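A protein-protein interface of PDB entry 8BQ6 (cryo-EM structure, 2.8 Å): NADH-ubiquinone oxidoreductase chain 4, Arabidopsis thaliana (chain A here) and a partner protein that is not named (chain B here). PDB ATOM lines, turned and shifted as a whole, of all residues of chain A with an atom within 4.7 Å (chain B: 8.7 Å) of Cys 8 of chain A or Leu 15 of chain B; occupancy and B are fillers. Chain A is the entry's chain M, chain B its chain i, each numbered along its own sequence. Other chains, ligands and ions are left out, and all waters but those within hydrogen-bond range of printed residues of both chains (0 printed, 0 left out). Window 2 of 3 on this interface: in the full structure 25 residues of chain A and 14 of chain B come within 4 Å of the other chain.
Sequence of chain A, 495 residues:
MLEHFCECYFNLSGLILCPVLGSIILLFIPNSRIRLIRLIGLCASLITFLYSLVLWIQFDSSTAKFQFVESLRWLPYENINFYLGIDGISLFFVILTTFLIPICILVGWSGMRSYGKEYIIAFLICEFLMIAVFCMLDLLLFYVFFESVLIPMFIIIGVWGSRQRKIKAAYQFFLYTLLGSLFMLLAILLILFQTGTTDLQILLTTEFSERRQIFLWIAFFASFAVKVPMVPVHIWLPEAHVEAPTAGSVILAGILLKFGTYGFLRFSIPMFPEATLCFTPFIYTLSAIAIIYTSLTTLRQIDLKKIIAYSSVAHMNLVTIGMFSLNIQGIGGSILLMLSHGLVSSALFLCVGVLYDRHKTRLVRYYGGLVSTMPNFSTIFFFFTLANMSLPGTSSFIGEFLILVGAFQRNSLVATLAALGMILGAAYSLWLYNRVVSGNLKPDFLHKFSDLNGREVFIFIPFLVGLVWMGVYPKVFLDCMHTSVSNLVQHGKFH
The side-chain sulfur (SG) of Cys 6 of chain A is in hydrogen-bond range of the side-chain carboxylate (OE1) of Glu 17 of chain B, at 3.5 Å. NZ of Lys 25 of chain B lies within salt-bridge range of OE2 of Glu 7 of chain A (3.3 Å). SG of Cys 8 of chain A lies within hydrogen-bond range of O of Leu 15 of chain B, at 3.1 Å. SG of Cys 8 of chain A is in hydrogen-bond range of N of Glu 17 of chain B, at 3.5 Å. N of Phe 68 of chain A is in hydrogen-bond range of OE2 of Glu 17 of chain B (2.8 Å).
The side-chain sulfur of Cys 6 of chain A sits at hydrogen-bond distance from the backbone NH of Cys 8 of chain A (3.5 Å). The backbone carbonyl oxygen (O) of Phe 10 of chain A is in hydrogen-bond range of the side-chain amide nitrogen (NE2) of Gln 58 of chain A (3.1 Å). The side-chain carboxylate (OE2) of Glu 17 of chain B lies within salt-bridge range of the guanidinium group (NE) of Arg 22 of chain B (3.9 Å).
C of Met 16 of chain B touches SG of Cys 8 of chain A, 3.99 Å away. CE2 of Phe 10 of chain A touches CD2 of Leu 15 of chain B (3.9 Å). Gln 58 of chain A touches Leu 15 of chain B.
Of the printed residues of chain B, Cys 6 of chain A touches Glu 17 (3.5 Å). Of the printed residues of chain B, Cys 8 of chain A touches Leu 15 (3.1 Å), Met 16 (3.99 Å) and Glu 17 (3.5 Å). Ala 8 of chain B touches none of the printed residues of chain A. Of chain A, only Cys 8 (3.1 Å), Phe 10 (3.9 Å) and Gln 58 (3.8 Å) come within 4 Å of Leu 15 of chain B. Of the printed residues of chain A, Met 16 of chain B touches Cys 8 (3.99 Å). The nearest residue of chain A that does not touch Leu 15 of chain B is Tyr 9 of chain A (4.2 Å). The nearest printed residue of chain A that does not touch Lys 25 of chain B is Cys 6 of chain A (4.5 Å).
Of the 13 printed residues of chain B, 4 touch a printed residue of chain A. Of the 7 printed residues of chain A, 6 touch a printed residue of chain B. Among the printed residues, Asp or Glu carboxylates within 4 Å of a Lys or Arg side-chain nitrogen of the other chain: Glu 7 of chain A with Lys 25 of chain B.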
ATOM      1  N   CYS A   6     -26.101  18.488   8.478  1.00  0.00           N
ATOM      2  CA  CYS A   6     -25.834  19.952   8.420  1.00  0.00           C
ATOM      3  C   CYS A   6     -24.404  20.242   7.942  1.00  0.00           C
ATOM      4  O   CYS A   6     -23.542  19.348   8.081  1.00  0.00           O
ATOM      5  CB  CYS A   6     -26.034  20.574   9.797  1.00  0.00           C
ATOM      6  SG  CYS A   6     -26.098  22.383   9.766  1.00  0.00           S
ATOM      7  N   GLU A   7     -24.159  21.456   7.432  1.00  0.00           N
ATOM      8  CA  GLU A   7     -22.806  21.861   6.952  1.00  0.00           C
ATOM      9  C   GLU A   7     -22.069  22.675   8.024  1.00  0.00           C
ATOM     10  O   GLU A   7     -20.850  22.876   7.851  1.00  0.00           O
ATOM     11  CB  GLU A   7     -22.928  22.660   5.655  1.00  0.00           C
ATOM     12  CG  GLU A   7     -23.575  21.884   4.518  1.00  0.00           C
ATOM     13  CD  GLU A   7     -25.039  22.184   4.230  1.00  0.00           C
ATOM     14  OE1 GLU A   7     -25.607  23.089   4.880  1.00  0.00           O
ATOM     15  OE2 GLU A   7     -25.611  21.507   3.354  1.00  0.00           O
ATOM     16  N   CYS A   8     -22.755  23.146   9.075  1.00  0.00           N
ATOM     17  CA  CYS A   8     -22.105  23.850  10.172  1.00  0.00           C
ATOM     18  C   CYS A   8     -21.140  22.931  10.919  1.00  0.00           C
ATOM     19  O   CYS A   8     -21.297  21.708  10.936  1.00  0.00           O
ATOM     20  CB  CYS A   8     -23.153  24.407  11.136  1.00  0.00           C
ATOM     21  SG  CYS A   8     -24.007  25.880  10.528  1.00  0.00           S
ATOM     22  N   TYR A   9     -20.126  23.540  11.540  1.00  0.00           N
ATOM     23  CA  TYR A   9     -19.154  22.777  12.322  1.00  0.00           C
ATOM     24  C   TYR A   9     -19.706  22.435  13.702  1.00  0.00           C
ATOM     25  O   TYR A   9     -19.633  21.285  14.150  1.00  0.00           O
ATOM     26  CB  TYR A   9     -17.835  23.549  12.454  1.00  0.00           C
ATOM     27  CG  TYR A   9     -17.218  24.049  11.160  1.00  0.00           C
ATOM     28  CD1 TYR A   9     -15.992  23.561  10.729  1.00  0.00           C
ATOM     29  CD2 TYR A   9     -17.836  25.026  10.391  1.00  0.00           C
ATOM     30  CE1 TYR A   9     -15.413  24.011   9.560  1.00  0.00           C
ATOM     31  CE2 TYR A   9     -17.266  25.481   9.222  1.00  0.00           C
ATOM     32  CZ  TYR A   9     -16.055  24.972   8.812  1.00  0.00           C
ATOM     33  OH  TYR A   9     -15.483  25.425   7.647  1.00  0.00           O
ATOM     34  N   PHE A  10     -20.244  23.434  14.399  1.00  0.00           N
ATOM     35  CA  PHE A  10     -20.944  23.210  15.659  1.00  0.00           C
ATOM     36  C   PHE A  10     -22.381  22.799  15.383  1.00  0.00           C
ATOM     37  O   PHE A  10     -23.161  23.583  14.834  1.00  0.00           O
ATOM     38  CB  PHE A  10     -20.921  24.476  16.509  1.00  0.00           C
ATOM     39  CG  PHE A  10     -19.550  25.002  16.780  1.00  0.00           C
ATOM     40  CD1 PHE A  10     -18.824  24.545  17.863  1.00  0.00           C
ATOM     41  CD2 PHE A  10     -18.970  25.928  15.934  1.00  0.00           C
ATOM     42  CE1 PHE A  10     -17.562  25.026  18.115  1.00  0.00           C
ATOM     43  CE2 PHE A  10     -17.706  26.407  16.180  1.00  0.00           C
ATOM     44  CZ  PHE A  10     -17.002  25.954  17.270  1.00  0.00           C
ATOM     45  N   GLN A  58     -24.276  31.476  15.598  1.00  0.00           N
ATOM     46  CA  GLN A  58     -24.498  31.163  14.191  1.00  0.00           C
ATOM     47  C   GLN A  58     -25.977  31.083  13.822  1.00  0.00           C
ATOM     48  O   GLN A  58     -26.310  30.625  12.722  1.00  0.00           O
ATOM     49  CB  GLN A  58     -23.802  29.855  13.829  1.00  0.00           C
ATOM     50  CG  GLN A  58     -23.874  28.837  14.927  1.00  0.00           C
ATOM     51  CD  GLN A  58     -23.334  27.503  14.502  1.00  0.00           C
ATOM     52  OE1 GLN A  58     -22.150  27.369  14.205  1.00  0.00           O
ATOM     53  NE2 GLN A  58     -24.199  26.499  14.476  1.00  0.00           N
ATOM     54  N   PHE A  68     -29.934  24.260  11.569  1.00  0.00           N
ATOM     55  CA  PHE A  68     -28.975  23.235  11.978  1.00  0.00           C
ATOM     56  C   PHE A  68     -29.589  21.843  11.919  1.00  0.00           C
ATOM     57  O   PHE A  68     -29.242  20.971  12.719  1.00  0.00           O
ATOM     58  CB  PHE A  68     -28.418  23.519  13.379  1.00  0.00           C
ATOM     59  CG  PHE A  68     -28.071  24.964  13.612  1.00  0.00           C
ATOM     60  CD1 PHE A  68     -27.358  25.681  12.669  1.00  0.00           C
ATOM     61  CD2 PHE A  68     -28.473  25.608  14.767  1.00  0.00           C
ATOM     62  CE1 PHE A  68     -27.049  27.005  12.878  1.00  0.00           C
ATOM     63  CE2 PHE A  68     -28.165  26.935  14.977  1.00  0.00           C
ATOM     64  CZ  PHE A  68     -27.454  27.631  14.032  1.00  0.00           C
ATOM     65  N   ALA B   8     -14.137  39.124  12.758  1.00  0.00           N
ATOM     66  CA  ALA B   8     -15.264  38.433  13.375  1.00  0.00           C
ATOM     67  C   ALA B   8     -16.471  38.394  12.446  1.00  0.00           C
ATOM     68  O   ALA B   8     -17.210  37.403  12.424  1.00  0.00           O
ATOM     69  CB  ALA B   8     -15.621  39.101  14.701  1.00  0.00           C
ATOM     70  N   GLU B   9     -16.696  39.466  11.681  1.00  0.00           N
ATOM     71  CA  GLU B   9     -17.763  39.455  10.683  1.00  0.00           C
ATOM     72  C   GLU B   9     -17.601  38.279   9.726  1.00  0.00           C
ATOM     73  O   GLU B   9     -18.542  37.510   9.503  1.00  0.00           O
ATOM     74  CB  GLU B   9     -17.782  40.781   9.914  1.00  0.00           C
ATOM     75  CG  GLU B   9     -17.915  42.024  10.795  1.00  0.00           C
ATOM     76  CD  GLU B   9     -19.353  42.433  11.072  1.00  0.00           C
ATOM     77  OE1 GLU B   9     -19.561  43.564  11.560  1.00  0.00           O
ATOM     78  OE2 GLU B   9     -20.275  41.652  10.769  1.00  0.00           O
ATOM     79  N   ASN B  10     -16.401  38.114   9.161  1.00  0.00           N
ATOM     80  CA  ASN B  10     -16.145  36.971   8.288  1.00  0.00           C
ATOM     81  C   ASN B  10     -16.258  35.657   9.046  1.00  0.00           C
ATOM     82  O   ASN B  10     -16.829  34.685   8.537  1.00  0.00           O
ATOM     83  CB  ASN B  10     -14.760  37.083   7.660  1.00  0.00           C
ATOM     84  CG  ASN B  10     -14.486  38.455   7.108  1.00  0.00           C
ATOM     85  OD1 ASN B  10     -15.334  39.053   6.447  1.00  0.00           O
ATOM     86  ND2 ASN B  10     -13.295  38.972   7.381  1.00  0.00           N
ATOM     87  N   LEU B  11     -15.705  35.605  10.260  1.00  0.00           N
ATOM     88  CA  LEU B  11     -15.686  34.353  11.006  1.00  0.00           C
ATOM     89  C   LEU B  11     -17.097  33.854  11.292  1.00  0.00           C
ATOM     90  O   LEU B  11     -17.380  32.660  11.141  1.00  0.00           O
ATOM     91  CB  LEU B  11     -14.908  34.527  12.308  1.00  0.00           C
ATOM     92  CG  LEU B  11     -14.857  33.256  13.158  1.00  0.00           C
ATOM     93  CD1 LEU B  11     -14.423  32.064  12.320  1.00  0.00           C
ATOM     94  CD2 LEU B  11     -13.949  33.433  14.358  1.00  0.00           C
ATOM     95  N   VAL B  12     -17.996  34.747  11.707  1.00  0.00           N
ATOM     96  CA  VAL B  12     -19.381  34.333  11.916  1.00  0.00           C
ATOM     97  C   VAL B  12     -20.026  33.943  10.594  1.00  0.00           C
ATOM     98  O   VAL B  12     -20.752  32.945  10.515  1.00  0.00           O
ATOM     99  CB  VAL B  12     -20.181  35.436  12.632  1.00  0.00           C
ATOM    100  CG1 VAL B  12     -21.587  34.949  12.899  1.00  0.00           C
ATOM    101  CG2 VAL B  12     -19.514  35.812  13.940  1.00  0.00           C
ATOM    102  N   LEU B  13     -19.777  34.722   9.537  1.00  0.00           N
ATOM    103  CA  LEU B  13     -20.355  34.412   8.229  1.00  0.00           C
ATOM    104  C   LEU B  13     -19.912  33.040   7.740  1.00  0.00           C
ATOM    105  O   LEU B  13     -20.679  32.331   7.079  1.00  0.00           O
ATOM    106  CB  LEU B  13     -19.965  35.484   7.214  1.00  0.00           C
ATOM    107  CG  LEU B  13     -20.754  36.791   7.167  1.00  0.00           C
ATOM    108  CD1 LEU B  13     -20.470  37.500   5.864  1.00  0.00           C
ATOM    109  CD2 LEU B  13     -22.239  36.525   7.307  1.00  0.00           C
ATOM    110  N   ARG B  14     -18.686  32.642   8.087  1.00  0.00           N
ATOM    111  CA  ARG B  14     -18.176  31.301   7.697  1.00  0.00           C
ATOM    112  C   ARG B  14     -18.901  30.215   8.495  1.00  0.00           C
ATOM    113  O   ARG B  14     -19.032  29.092   7.970  1.00  0.00           O
ATOM    114  CB  ARG B  14     -16.674  31.211   7.974  1.00  0.00           C
ATOM    115  CG  ARG B  14     -15.894  30.424   6.933  1.00  0.00           C
ATOM    116  CD  ARG B  14     -14.490  30.969   6.769  1.00  0.00           C
ATOM    117  NE  ARG B  14     -14.464  32.164   5.938  1.00  0.00           N
ATOM    118  CZ  ARG B  14     -14.114  33.375   6.357  1.00  0.00           C
ATOM    119  NH1 ARG B  14     -13.752  33.568   7.613  1.00  0.00           N
ATOM    120  NH2 ARG B  14     -14.127  34.390   5.513  1.00  0.00           N
ATOM    121  N   LEU B  15     -19.361  30.536   9.707  1.00  0.00           N
ATOM    122  CA  LEU B  15     -19.976  29.530  10.565  1.00  0.00           C
ATOM    123  C   LEU B  15     -21.442  29.280  10.235  1.00  0.00           C
ATOM    124  O   LEU B  15     -21.938  28.180  10.493  1.00  0.00           O
ATOM    125  CB  LEU B  15     -19.838  29.947  12.027  1.00  0.00           C
ATOM    126  CG  LEU B  15     -18.447  29.866  12.651  1.00  0.00           C
ATOM    127  CD1 LEU B  15     -18.447  30.571  13.990  1.00  0.00           C
ATOM    128  CD2 LEU B  15     -18.022  28.420  12.813  1.00  0.00           C
ATOM    129  N   MET B  16     -22.146  30.268   9.687  1.00  0.00           N
ATOM    130  CA  MET B  16     -23.566  30.108   9.401  1.00  0.00           C
ATOM    131  C   MET B  16     -23.773  29.140   8.242  1.00  0.00           C
ATOM    132  O   MET B  16     -22.939  29.041   7.340  1.00  0.00           O
ATOM    133  CB  MET B  16     -24.200  31.458   9.068  1.00  0.00           C
ATOM    134  CG  MET B  16     -23.704  32.607   9.918  1.00  0.00           C
ATOM    135  SD  MET B  16     -24.746  34.072   9.820  1.00  0.00           S
ATOM    136  CE  MET B  16     -25.044  34.396  11.554  1.00  0.00           C
ATOM    137  N   GLU B  17     -24.892  28.420   8.270  1.00  0.00           N
ATOM    138  CA  GLU B  17     -25.200  27.510   7.180  1.00  0.00           C
ATOM    139  C   GLU B  17     -25.695  28.293   5.964  1.00  0.00           C
ATOM    140  O   GLU B  17     -26.181  29.422   6.071  1.00  0.00           O
ATOM    141  CB  GLU B  17     -26.231  26.466   7.621  1.00  0.00           C
ATOM    142  CG  GLU B  17     -27.514  27.035   8.197  1.00  0.00           C
ATOM    143  CD  GLU B  17     -28.376  25.978   8.872  1.00  0.00           C
ATOM    144  OE1 GLU B  17     -28.306  24.796   8.471  1.00  0.00           O
ATOM    145  OE2 GLU B  17     -29.130  26.336   9.801  1.00  0.00           O
ATOM    146  N   ASN B  18     -25.548  27.687   4.791  1.00  0.00           N
ATOM    147  CA  ASN B  18     -25.962  28.329   3.548  1.00  0.00           C
ATOM    148  C   ASN B  18     -27.483  28.379   3.466  1.00  0.00           C
ATOM    149  O   ASN B  18     -28.132  27.334   3.582  1.00  0.00           O
ATOM    150  CB  ASN B  18     -25.400  27.576   2.351  1.00  0.00           C
ATOM    151  CG  ASN B  18     -25.319  28.435   1.109  1.00  0.00           C
ATOM    152  OD1 ASN B  18     -25.115  29.646   1.188  1.00  0.00           O
ATOM    153  ND2 ASN B  18     -25.484  27.812  -0.048  1.00  0.00           N
ATOM    154  N   ARG B  22     -29.992  25.052   2.698  1.00  0.00           N
ATOM    155  CA  ARG B  22     -30.830  24.717   3.842  1.00  0.00           C
ATOM    156  C   ARG B  22     -32.305  24.716   3.456  1.00  0.00           C
ATOM    157  O   ARG B  22     -33.067  23.840   3.879  1.00  0.00           O
ATOM    158  CB  ARG B  22     -30.557  25.699   4.981  1.00  0.00           C
ATOM    159  CG  ARG B  22     -31.277  25.373   6.267  1.00  0.00           C
ATOM    160  CD  ARG B  22     -32.228  26.485   6.665  1.00  0.00           C
ATOM    161  NE  ARG B  22     -31.522  27.689   7.087  1.00  0.00           N
ATOM    162  CZ  ARG B  22     -31.673  28.881   6.527  1.00  0.00           C
ATOM    163  NH1 ARG B  22     -32.511  29.071   5.521  1.00  0.00           N
ATOM    164  NH2 ARG B  22     -30.973  29.910   6.993  1.00  0.00           N
ATOM    165  N   LYS B  25     -32.941  21.558   0.930  1.00  0.00           N
ATOM    166  CA  LYS B  25     -33.089  20.255   1.629  1.00  0.00           C
ATOM    167  C   LYS B  25     -34.426  20.205   2.379  1.00  0.00           C
ATOM    168  O   LYS B  25     -35.023  19.123   2.412  1.00  0.00           O
ATOM    169  CB  LYS B  25     -31.889  20.031   2.551  1.00  0.00           C
ATOM    170  CG  LYS B  25     -30.599  19.614   1.860  1.00  0.00           C
ATOM    171  CD  LYS B  25     -29.423  19.522   2.806  1.00  0.00           C
ATOM    172  CE  LYS B  25     -29.196  20.790   3.600  1.00  0.00           C
ATOM    173  NZ  LYS B  25     -28.372  20.545   4.807  1.00  0.00           N
